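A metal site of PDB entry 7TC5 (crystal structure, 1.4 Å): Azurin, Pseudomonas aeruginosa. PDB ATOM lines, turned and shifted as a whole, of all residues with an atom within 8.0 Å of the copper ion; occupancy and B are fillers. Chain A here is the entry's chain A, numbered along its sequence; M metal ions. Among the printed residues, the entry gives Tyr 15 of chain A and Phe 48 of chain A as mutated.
ND1 of His 117 binds the copper ion (2.0 Å).
The copper ion is bound by ND1 of His 46, at 2.0 Å.
The side-chain sulfur (SG) of Cys 112 binds the copper ion (2.2 Å).
The copper ion has three donor atoms within binding distance.
Merely in contact with the copper ion: Gly 45 (3.0 Å), Met 121 (3.3 Å) and Phe 114 (3.8 Å).
SD of Met 121 lies close to ND1 of His 46 (3.3 Å).
NE2 of His 46 sits at hydrogen-bond distance from O of Asn 10 (2.8 Å).
The backbone carbonyl oxygen of His 46 sits at hydrogen-bond distance from the backbone NH of Ile 87 (2.8 Å).
The backbone NH of Cys 112 lies within hydrogen-bond range of the backbone carbonyl oxygen of Met 121.
N of Phe 114 lies close to SG of Cys 112, at 3.4 Å.
The side-chain sulfur (SG) of Cys 112 lies close to the backbone NH (N) of Asn 47 (3.5 Å).
The backbone NH (N) of Cys 112 lies within hydrogen-bond range of the side-chain hydroxyl (OH) of Tyr 15 (3.1 Å).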
ATOM      1  N   GLY A   9      20.718  21.335 -14.062  1.00  0.00           N
ATOM      2  CA  GLY A   9      21.718  20.543 -14.756  1.00  0.00           C
ATOM      3  C   GLY A   9      22.994  20.559 -13.954  1.00  0.00           C
ATOM      4  O   GLY A   9      23.411  21.643 -13.505  1.00  0.00           O
ATOM      5  N   ASN A  10      23.644  19.432 -13.873  1.00  0.00           N
ATOM      6  CA  ASN A  10      24.733  19.288 -12.882  1.00  0.00           C
ATOM      7  C   ASN A  10      26.076  18.978 -13.528  1.00  0.00           C
ATOM      8  O   ASN A  10      26.224  18.993 -14.759  1.00  0.00           O
ATOM      9  CB  ASN A  10      24.298  18.265 -11.834  1.00  0.00           C
ATOM     10  CG  ASN A  10      24.226  16.846 -12.322  1.00  0.00           C
ATOM     11  OD1 ASN A  10      24.652  16.533 -13.433  1.00  0.00           O
ATOM     12  ND2 ASN A  10      23.699  15.980 -11.478  1.00  0.00           N
ATOM     13  N   MET A  13      26.392  15.871 -16.052  1.00  0.00           N
ATOM     14  CA  MET A  13      25.708  15.946 -17.362  1.00  0.00           C
ATOM     15  C   MET A  13      24.300  15.358 -17.234  1.00  0.00           C
ATOM     16  O   MET A  13      23.838  14.639 -18.123  1.00  0.00           O
ATOM     17  CB  MET A  13      26.510  15.195 -18.424  1.00  0.00           C
ATOM     18  CG  MET A  13      26.313  15.741 -19.801  1.00  0.00           C
ATOM     19  SD  MET A  13      27.153  14.711 -21.066  1.00  0.00           S
ATOM     20  CE  MET A  13      25.962  13.419 -21.311  1.00  0.00           C
ATOM     21  N   GLN A  14      23.612  15.662 -16.147  1.00  0.00           N
ATOM     22  CA  GLN A  14      22.228  15.201 -15.929  1.00  0.00           C
ATOM     23  C   GLN A  14      21.317  16.389 -15.702  1.00  0.00           C
ATOM     24  O   GLN A  14      21.669  17.341 -14.982  1.00  0.00           O
ATOM     25  CB  GLN A  14      22.117  14.376 -14.660  1.00  0.00           C
ATOM     26  CG  GLN A  14      22.909  13.092 -14.649  1.00  0.00           C
ATOM     27  CD  GLN A  14      22.952  12.501 -13.253  1.00  0.00           C
ATOM     28  OE1 GLN A  14      22.991  13.215 -12.258  1.00  0.00           O
ATOM     29  NE2 GLN A  14      22.915  11.185 -13.183  1.00  0.00           N
ATOM     30  N   TYR A  15      20.087  16.269 -16.193  1.00  0.00           N
ATOM     31  CA  TYR A  15      19.003  17.105 -15.699  1.00  0.00           C
ATOM     32  C   TYR A  15      18.408  16.382 -14.489  1.00  0.00           C
ATOM     33  O   TYR A  15      18.470  15.116 -14.479  1.00  0.00           O
ATOM     34  CB  TYR A  15      17.866  17.250 -16.714  1.00  0.00           C
ATOM     35  CG  TYR A  15      18.030  18.226 -17.853  1.00  0.00           C
ATOM     36  CD1 TYR A  15      18.564  19.496 -17.713  1.00  0.00           C
ATOM     37  CD2 TYR A  15      17.608  17.852 -19.123  1.00  0.00           C
ATOM     38  CE1 TYR A  15      18.631  20.396 -18.777  1.00  0.00           C
ATOM     39  CE2 TYR A  15      17.677  18.732 -20.195  1.00  0.00           C
ATOM     40  CZ  TYR A  15      18.117  20.027 -20.004  1.00  0.00           C
ATOM     41  OH  TYR A  15      18.141  20.888 -21.062  1.00  0.00           O
ATOM     42  N   LEU A  33      15.923  27.276 -14.951  1.00  0.00           N
ATOM     43  CA  LEU A  33      17.108  26.398 -15.000  1.00  0.00           C
ATOM     44  C   LEU A  33      18.160  26.928 -14.025  1.00  0.00           C
ATOM     45  O   LEU A  33      18.430  28.135 -14.019  1.00  0.00           O
ATOM     46  CB  LEU A  33      17.662  26.420 -16.432  1.00  0.00           C
ATOM     47  CG  LEU A  33      18.869  25.508 -16.639  1.00  0.00           C
ATOM     48  CD1 LEU A  33      18.533  24.046 -16.532  1.00  0.00           C
ATOM     49  CD2 LEU A  33      19.517  25.798 -18.010  1.00  0.00           C
ATOM     50  N   HIS A  35      22.263  25.546 -12.277  1.00  0.00           N
ATOM     51  CA  HIS A  35      23.437  24.662 -12.449  1.00  0.00           C
ATOM     52  C   HIS A  35      24.199  24.526 -11.137  1.00  0.00           C
ATOM     53  O   HIS A  35      25.124  25.267 -10.894  1.00  0.00           O
ATOM     54  CB  HIS A  35      24.298  25.246 -13.550  1.00  0.00           C
ATOM     55  CG  HIS A  35      25.419  24.390 -14.009  1.00  0.00           C
ATOM     56  ND1 HIS A  35      26.104  23.471 -13.230  1.00  0.00           N
ATOM     57  CD2 HIS A  35      25.993  24.348 -15.243  1.00  0.00           C
ATOM     58  CE1 HIS A  35      27.023  22.892 -13.987  1.00  0.00           C
ATOM     59  NE2 HIS A  35      26.977  23.408 -15.200  1.00  0.00           N
ATOM     60  N   LYS A  41      31.079  27.219 -17.661  1.00  0.00           N
ATOM     61  CA  LYS A  41      30.195  27.168 -18.822  1.00  0.00           C
ATOM     62  C   LYS A  41      30.940  26.583 -20.030  1.00  0.00           C
ATOM     63  O   LYS A  41      30.273  25.935 -20.838  1.00  0.00           O
ATOM     64  CB  LYS A  41      29.769  28.601 -19.139  1.00  0.00           C
ATOM     65  CG  LYS A  41      28.764  28.736 -20.251  1.00  0.00           C
ATOM     66  CD  LYS A  41      28.373  30.168 -20.458  1.00  0.00           C
ATOM     67  CE  LYS A  41      29.373  30.883 -21.301  1.00  0.00           C
ATOM     68  NZ  LYS A  41      28.768  32.095 -21.947  1.00  0.00           N
ATOM     69  N   VAL A  43      33.047  24.268 -20.270  1.00  0.00           N
ATOM     70  CA  VAL A  43      33.302  22.808 -20.172  1.00  0.00           C
ATOM     71  C   VAL A  43      32.073  22.006 -19.820  1.00  0.00           C
ATOM     72  O   VAL A  43      32.058  20.841 -20.155  1.00  0.00           O
ATOM     73  CB  VAL A  43      34.453  22.485 -19.213  1.00  0.00           C
ATOM     74  CG1 VAL A  43      35.643  23.373 -19.485  1.00  0.00           C
ATOM     75  CG2 VAL A  43      34.040  22.563 -17.786  1.00  0.00           C
ATOM     76  N   MET A  44      31.116  22.602 -19.143  1.00  0.00           N
ATOM     77  CA  MET A  44      29.927  21.886 -18.630  1.00  0.00           C
ATOM     78  C   MET A  44      28.745  22.854 -18.666  1.00  0.00           C
ATOM     79  O   MET A  44      27.929  22.840 -17.768  1.00  0.00           O
ATOM     80  CB  MET A  44      30.136  21.370 -17.202  1.00  0.00           C
ATOM     81  CG  MET A  44      29.095  20.327 -16.728  1.00  0.00           C
ATOM     82  SD  MET A  44      28.802  18.850 -17.769  1.00  0.00           S
ATOM     83  CE  MET A  44      30.274  17.872 -17.428  1.00  0.00           C
ATOM     84  N   GLY A  45      28.685  23.740 -19.632  1.00  0.00           N
ATOM     85  CA  GLY A  45      27.554  24.668 -19.728  1.00  0.00           C
ATOM     86  C   GLY A  45      26.281  23.921 -20.071  1.00  0.00           C
ATOM     87  O   GLY A  45      26.361  22.928 -20.837  1.00  0.00           O
ATOM     88  N   HIS A  46      25.160  24.364 -19.535  1.00  0.00           N
ATOM     89  CA  HIS A  46      23.868  23.756 -19.833  1.00  0.00           C
ATOM     90  C   HIS A  46      22.871  24.802 -20.258  1.00  0.00           C
ATOM     91  O   HIS A  46      22.862  25.888 -19.733  1.00  0.00           O
ATOM     92  CB  HIS A  46      23.253  22.990 -18.640  1.00  0.00           C
ATOM     93  CG  HIS A  46      24.156  21.925 -18.099  1.00  0.00           C
ATOM     94  ND1 HIS A  46      24.717  20.979 -18.902  1.00  0.00           N
ATOM     95  CD2 HIS A  46      24.511  21.653 -16.824  1.00  0.00           C
ATOM     96  CE1 HIS A  46      25.434  20.162 -18.159  1.00  0.00           C
ATOM     97  NE2 HIS A  46      25.287  20.553 -16.847  1.00  0.00           N
ATOM     98  N   ASN A  47      22.004  24.397 -21.169  1.00  0.00           N
ATOM     99  CA  ASN A  47      20.822  25.188 -21.484  1.00  0.00           C
ATOM    100  C   ASN A  47      19.620  24.288 -21.360  1.00  0.00           C
ATOM    101  O   ASN A  47      19.741  23.097 -21.168  1.00  0.00           O
ATOM    102  CB  ASN A  47      21.031  25.981 -22.774  1.00  0.00           C
ATOM    103  CG  ASN A  47      21.286  25.108 -23.967  1.00  0.00           C
ATOM    104  OD1 ASN A  47      21.052  23.906 -23.952  1.00  0.00           O
ATOM    105  ND2 ASN A  47      21.739  25.721 -25.059  1.00  0.00           N
ATOM    106  N   PHE A  48      18.498  24.873 -21.612  1.00  0.00           N
ATOM    107  CA  PHE A  48      17.197  24.215 -21.728  1.00  0.00           C
ATOM    108  C   PHE A  48      16.599  24.752 -23.022  1.00  0.00           C
ATOM    109  O   PHE A  48      16.363  25.960 -23.134  1.00  0.00           O
ATOM    110  CB  PHE A  48      16.265  24.573 -20.560  1.00  0.00           C
ATOM    111  CG  PHE A  48      14.864  24.011 -20.713  1.00  0.00           C
ATOM    112  CD1 PHE A  48      13.913  24.705 -21.440  1.00  0.00           C
ATOM    113  CD2 PHE A  48      14.473  22.825 -20.108  1.00  0.00           C
ATOM    114  CE1 PHE A  48      12.612  24.219 -21.555  1.00  0.00           C
ATOM    115  CE2 PHE A  48      13.171  22.324 -20.261  1.00  0.00           C
ATOM    116  CZ  PHE A  48      12.268  23.030 -20.971  1.00  0.00           C
ATOM    117  N   LEU A  86      22.916  29.483 -22.128  1.00  0.00           N
ATOM    118  CA  LEU A  86      23.865  28.461 -21.673  1.00  0.00           C
ATOM    119  C   LEU A  86      24.480  28.983 -20.357  1.00  0.00           C
ATOM    120  O   LEU A  86      24.964  30.110 -20.347  1.00  0.00           O
ATOM    121  CB  LEU A  86      24.926  28.254 -22.744  1.00  0.00           C
ATOM    122  CG  LEU A  86      25.824  27.069 -22.541  1.00  0.00           C
ATOM    123  CD1 LEU A  86      25.114  25.783 -22.894  1.00  0.00           C
ATOM    124  CD2 LEU A  86      27.093  27.236 -23.347  1.00  0.00           C
ATOM    125  N   ILE A  87      24.341  28.225 -19.282  1.00  0.00           N
ATOM    126  CA  ILE A  87      24.795  28.684 -17.950  1.00  0.00           C
ATOM    127  C   ILE A  87      25.883  27.767 -17.464  1.00  0.00           C
ATOM    128  O   ILE A  87      25.844  26.554 -17.667  1.00  0.00           O
ATOM    129  CB  ILE A  87      23.642  28.798 -16.962  1.00  0.00           C
ATOM    130  CG1 ILE A  87      22.932  27.452 -16.740  1.00  0.00           C
ATOM    131  CG2 ILE A  87      22.690  29.905 -17.398  1.00  0.00           C
ATOM    132  CD1 ILE A  87      21.910  27.444 -15.576  1.00  0.00           C
ATOM    133  N   PHE A 111      15.989  19.702 -24.146  1.00  0.00           N
ATOM    134  CA  PHE A 111      17.359  19.151 -24.165  1.00  0.00           C
ATOM    135  C   PHE A 111      18.348  20.286 -24.022  1.00  0.00           C
ATOM    136  O   PHE A 111      18.049  21.459 -24.233  1.00  0.00           O
ATOM    137  CB  PHE A 111      17.593  18.410 -25.509  1.00  0.00           C
ATOM    138  CG  PHE A 111      17.082  19.168 -26.708  1.00  0.00           C
ATOM    139  CD1 PHE A 111      17.904  20.077 -27.371  1.00  0.00           C
ATOM    140  CD2 PHE A 111      15.788  19.012 -27.171  1.00  0.00           C
ATOM    141  CE1 PHE A 111      17.443  20.809 -28.464  1.00  0.00           C
ATOM    142  CE2 PHE A 111      15.301  19.825 -28.179  1.00  0.00           C
ATOM    143  CZ  PHE A 111      16.132  20.680 -28.864  1.00  0.00           C
ATOM    144  N   CYS A 112      19.571  19.896 -23.679  1.00  0.00           N
ATOM    145  CA  CYS A 112      20.749  20.761 -23.679  1.00  0.00           C
ATOM    146  C   CYS A 112      21.503  20.615 -25.005  1.00  0.00           C
ATOM    147  O   CYS A 112      21.742  19.449 -25.430  1.00  0.00           O
ATOM    148  CB  CYS A 112      21.616  20.423 -22.483  1.00  0.00           C
ATOM    149  SG  CYS A 112      23.138  21.392 -22.439  1.00  0.00           S
ATOM    150  N   THR A 113      21.902  21.720 -25.596  1.00  0.00           N
ATOM    151  CA  THR A 113      22.608  21.652 -26.897  1.00  0.00           C
ATOM    152  C   THR A 113      24.133  21.741 -26.709  1.00  0.00           C
ATOM    153  O   THR A 113      24.847  21.781 -27.724  1.00  0.00           O
ATOM    154  CB  THR A 113      22.114  22.755 -27.825  1.00  0.00           C
ATOM    155  OG1 THR A 113      22.368  24.039 -27.257  1.00  0.00           O
ATOM    156  CG2 THR A 113      20.651  22.584 -28.161  1.00  0.00           C
ATOM    157  N   PHE A 114      24.666  21.794 -25.505  1.00  0.00           N
ATOM    158  CA  PHE A 114      26.138  21.671 -25.354  1.00  0.00           C
ATOM    159  C   PHE A 114      26.517  20.342 -26.001  1.00  0.00           C
ATOM    160  O   PHE A 114      25.899  19.309 -25.723  1.00  0.00           O
ATOM    161  CB  PHE A 114      26.574  21.757 -23.890  1.00  0.00           C
ATOM    162  CG  PHE A 114      28.058  21.982 -23.717  1.00  0.00           C
ATOM    163  CD1 PHE A 114      28.975  20.982 -23.986  1.00  0.00           C
ATOM    164  CD2 PHE A 114      28.535  23.219 -23.277  1.00  0.00           C
ATOM    165  CE1 PHE A 114      30.349  21.222 -23.851  1.00  0.00           C
ATOM    166  CE2 PHE A 114      29.889  23.430 -23.120  1.00  0.00           C
ATOM    167  CZ  PHE A 114      30.788  22.431 -23.357  1.00  0.00           C
ATOM    168  N   PRO A 115      27.495  20.289 -26.913  1.00  0.00           N
ATOM    169  CA  PRO A 115      27.742  19.047 -27.655  1.00  0.00           C
ATOM    170  C   PRO A 115      27.979  17.854 -26.724  1.00  0.00           C
ATOM    171  O   PRO A 115      28.765  17.941 -25.805  1.00  0.00           O
ATOM    172  CB  PRO A 115      28.887  19.369 -28.594  1.00  0.00           C
ATOM    173  CG  PRO A 115      28.672  20.881 -28.818  1.00  0.00           C
ATOM    174  CD  PRO A 115      28.275  21.403 -27.430  1.00  0.00           C
ATOM    175  N   GLY A 116      27.317  16.740 -27.051  1.00  0.00           N
ATOM    176  CA  GLY A 116      27.369  15.493 -26.286  1.00  0.00           C
ATOM    177  C   GLY A 116      26.345  15.444 -25.193  1.00  0.00           C
ATOM    178  O   GLY A 116      26.030  14.347 -24.751  1.00  0.00           O
ATOM    179  N   HIS A 117      25.853  16.580 -24.745  1.00  0.00           N
ATOM    180  CA  HIS A 117      25.050  16.552 -23.491  1.00  0.00           C
ATOM    181  C   HIS A 117      23.679  15.923 -23.750  1.00  0.00           C
ATOM    182  O   HIS A 117      23.127  15.360 -22.802  1.00  0.00           O
ATOM    183  CB  HIS A 117      24.882  17.930 -22.887  1.00  0.00           C
ATOM    184  CG  HIS A 117      26.113  18.425 -22.256  1.00  0.00           C
ATOM    185  ND1 HIS A 117      26.113  19.471 -21.347  1.00  0.00           N
ATOM    186  CD2 HIS A 117      27.392  18.028 -22.412  1.00  0.00           C
ATOM    187  CE1 HIS A 117      27.359  19.684 -20.981  1.00  0.00           C
ATOM    188  NE2 HIS A 117      28.161  18.797 -21.584  1.00  0.00           N
ATOM    189  N   SER A 118      23.107  16.075 -24.934  1.00  0.00           N
ATOM    190  CA  SER A 118      21.731  15.603 -25.217  1.00  0.00           C
ATOM    191  C   SER A 118      21.606  14.080 -25.143  1.00  0.00           C
ATOM    192  O   SER A 118      20.455  13.615 -25.076  1.00  0.00           O
ATOM    193  CB  SER A 118      21.182  16.162 -26.432  1.00  0.00           C
ATOM    194  OG  SER A 118      21.895  15.733 -27.539  1.00  0.00           O
ATOM    195  N   MET A 121      20.938  14.601 -21.329  1.00  0.00           N
ATOM    196  CA  MET A 121      20.203  15.833 -20.924  1.00  0.00           C
ATOM    197  C   MET A 121      19.101  16.087 -21.952  1.00  0.00           C
ATOM    198  O   MET A 121      19.235  16.900 -22.847  1.00  0.00           O
ATOM    199  CB  MET A 121      21.109  17.038 -20.755  1.00  0.00           C
ATOM    200  CG  MET A 121      22.168  16.719 -19.753  1.00  0.00           C
ATOM    201  SD  MET A 121      23.201  18.088 -19.320  1.00  0.00           S
ATOM    202  CE  MET A 121      22.051  19.152 -18.455  1.00  0.00           C
HETATM  203 CU    CU M   1      24.493  20.620 -20.898  1.00  0.00          CU
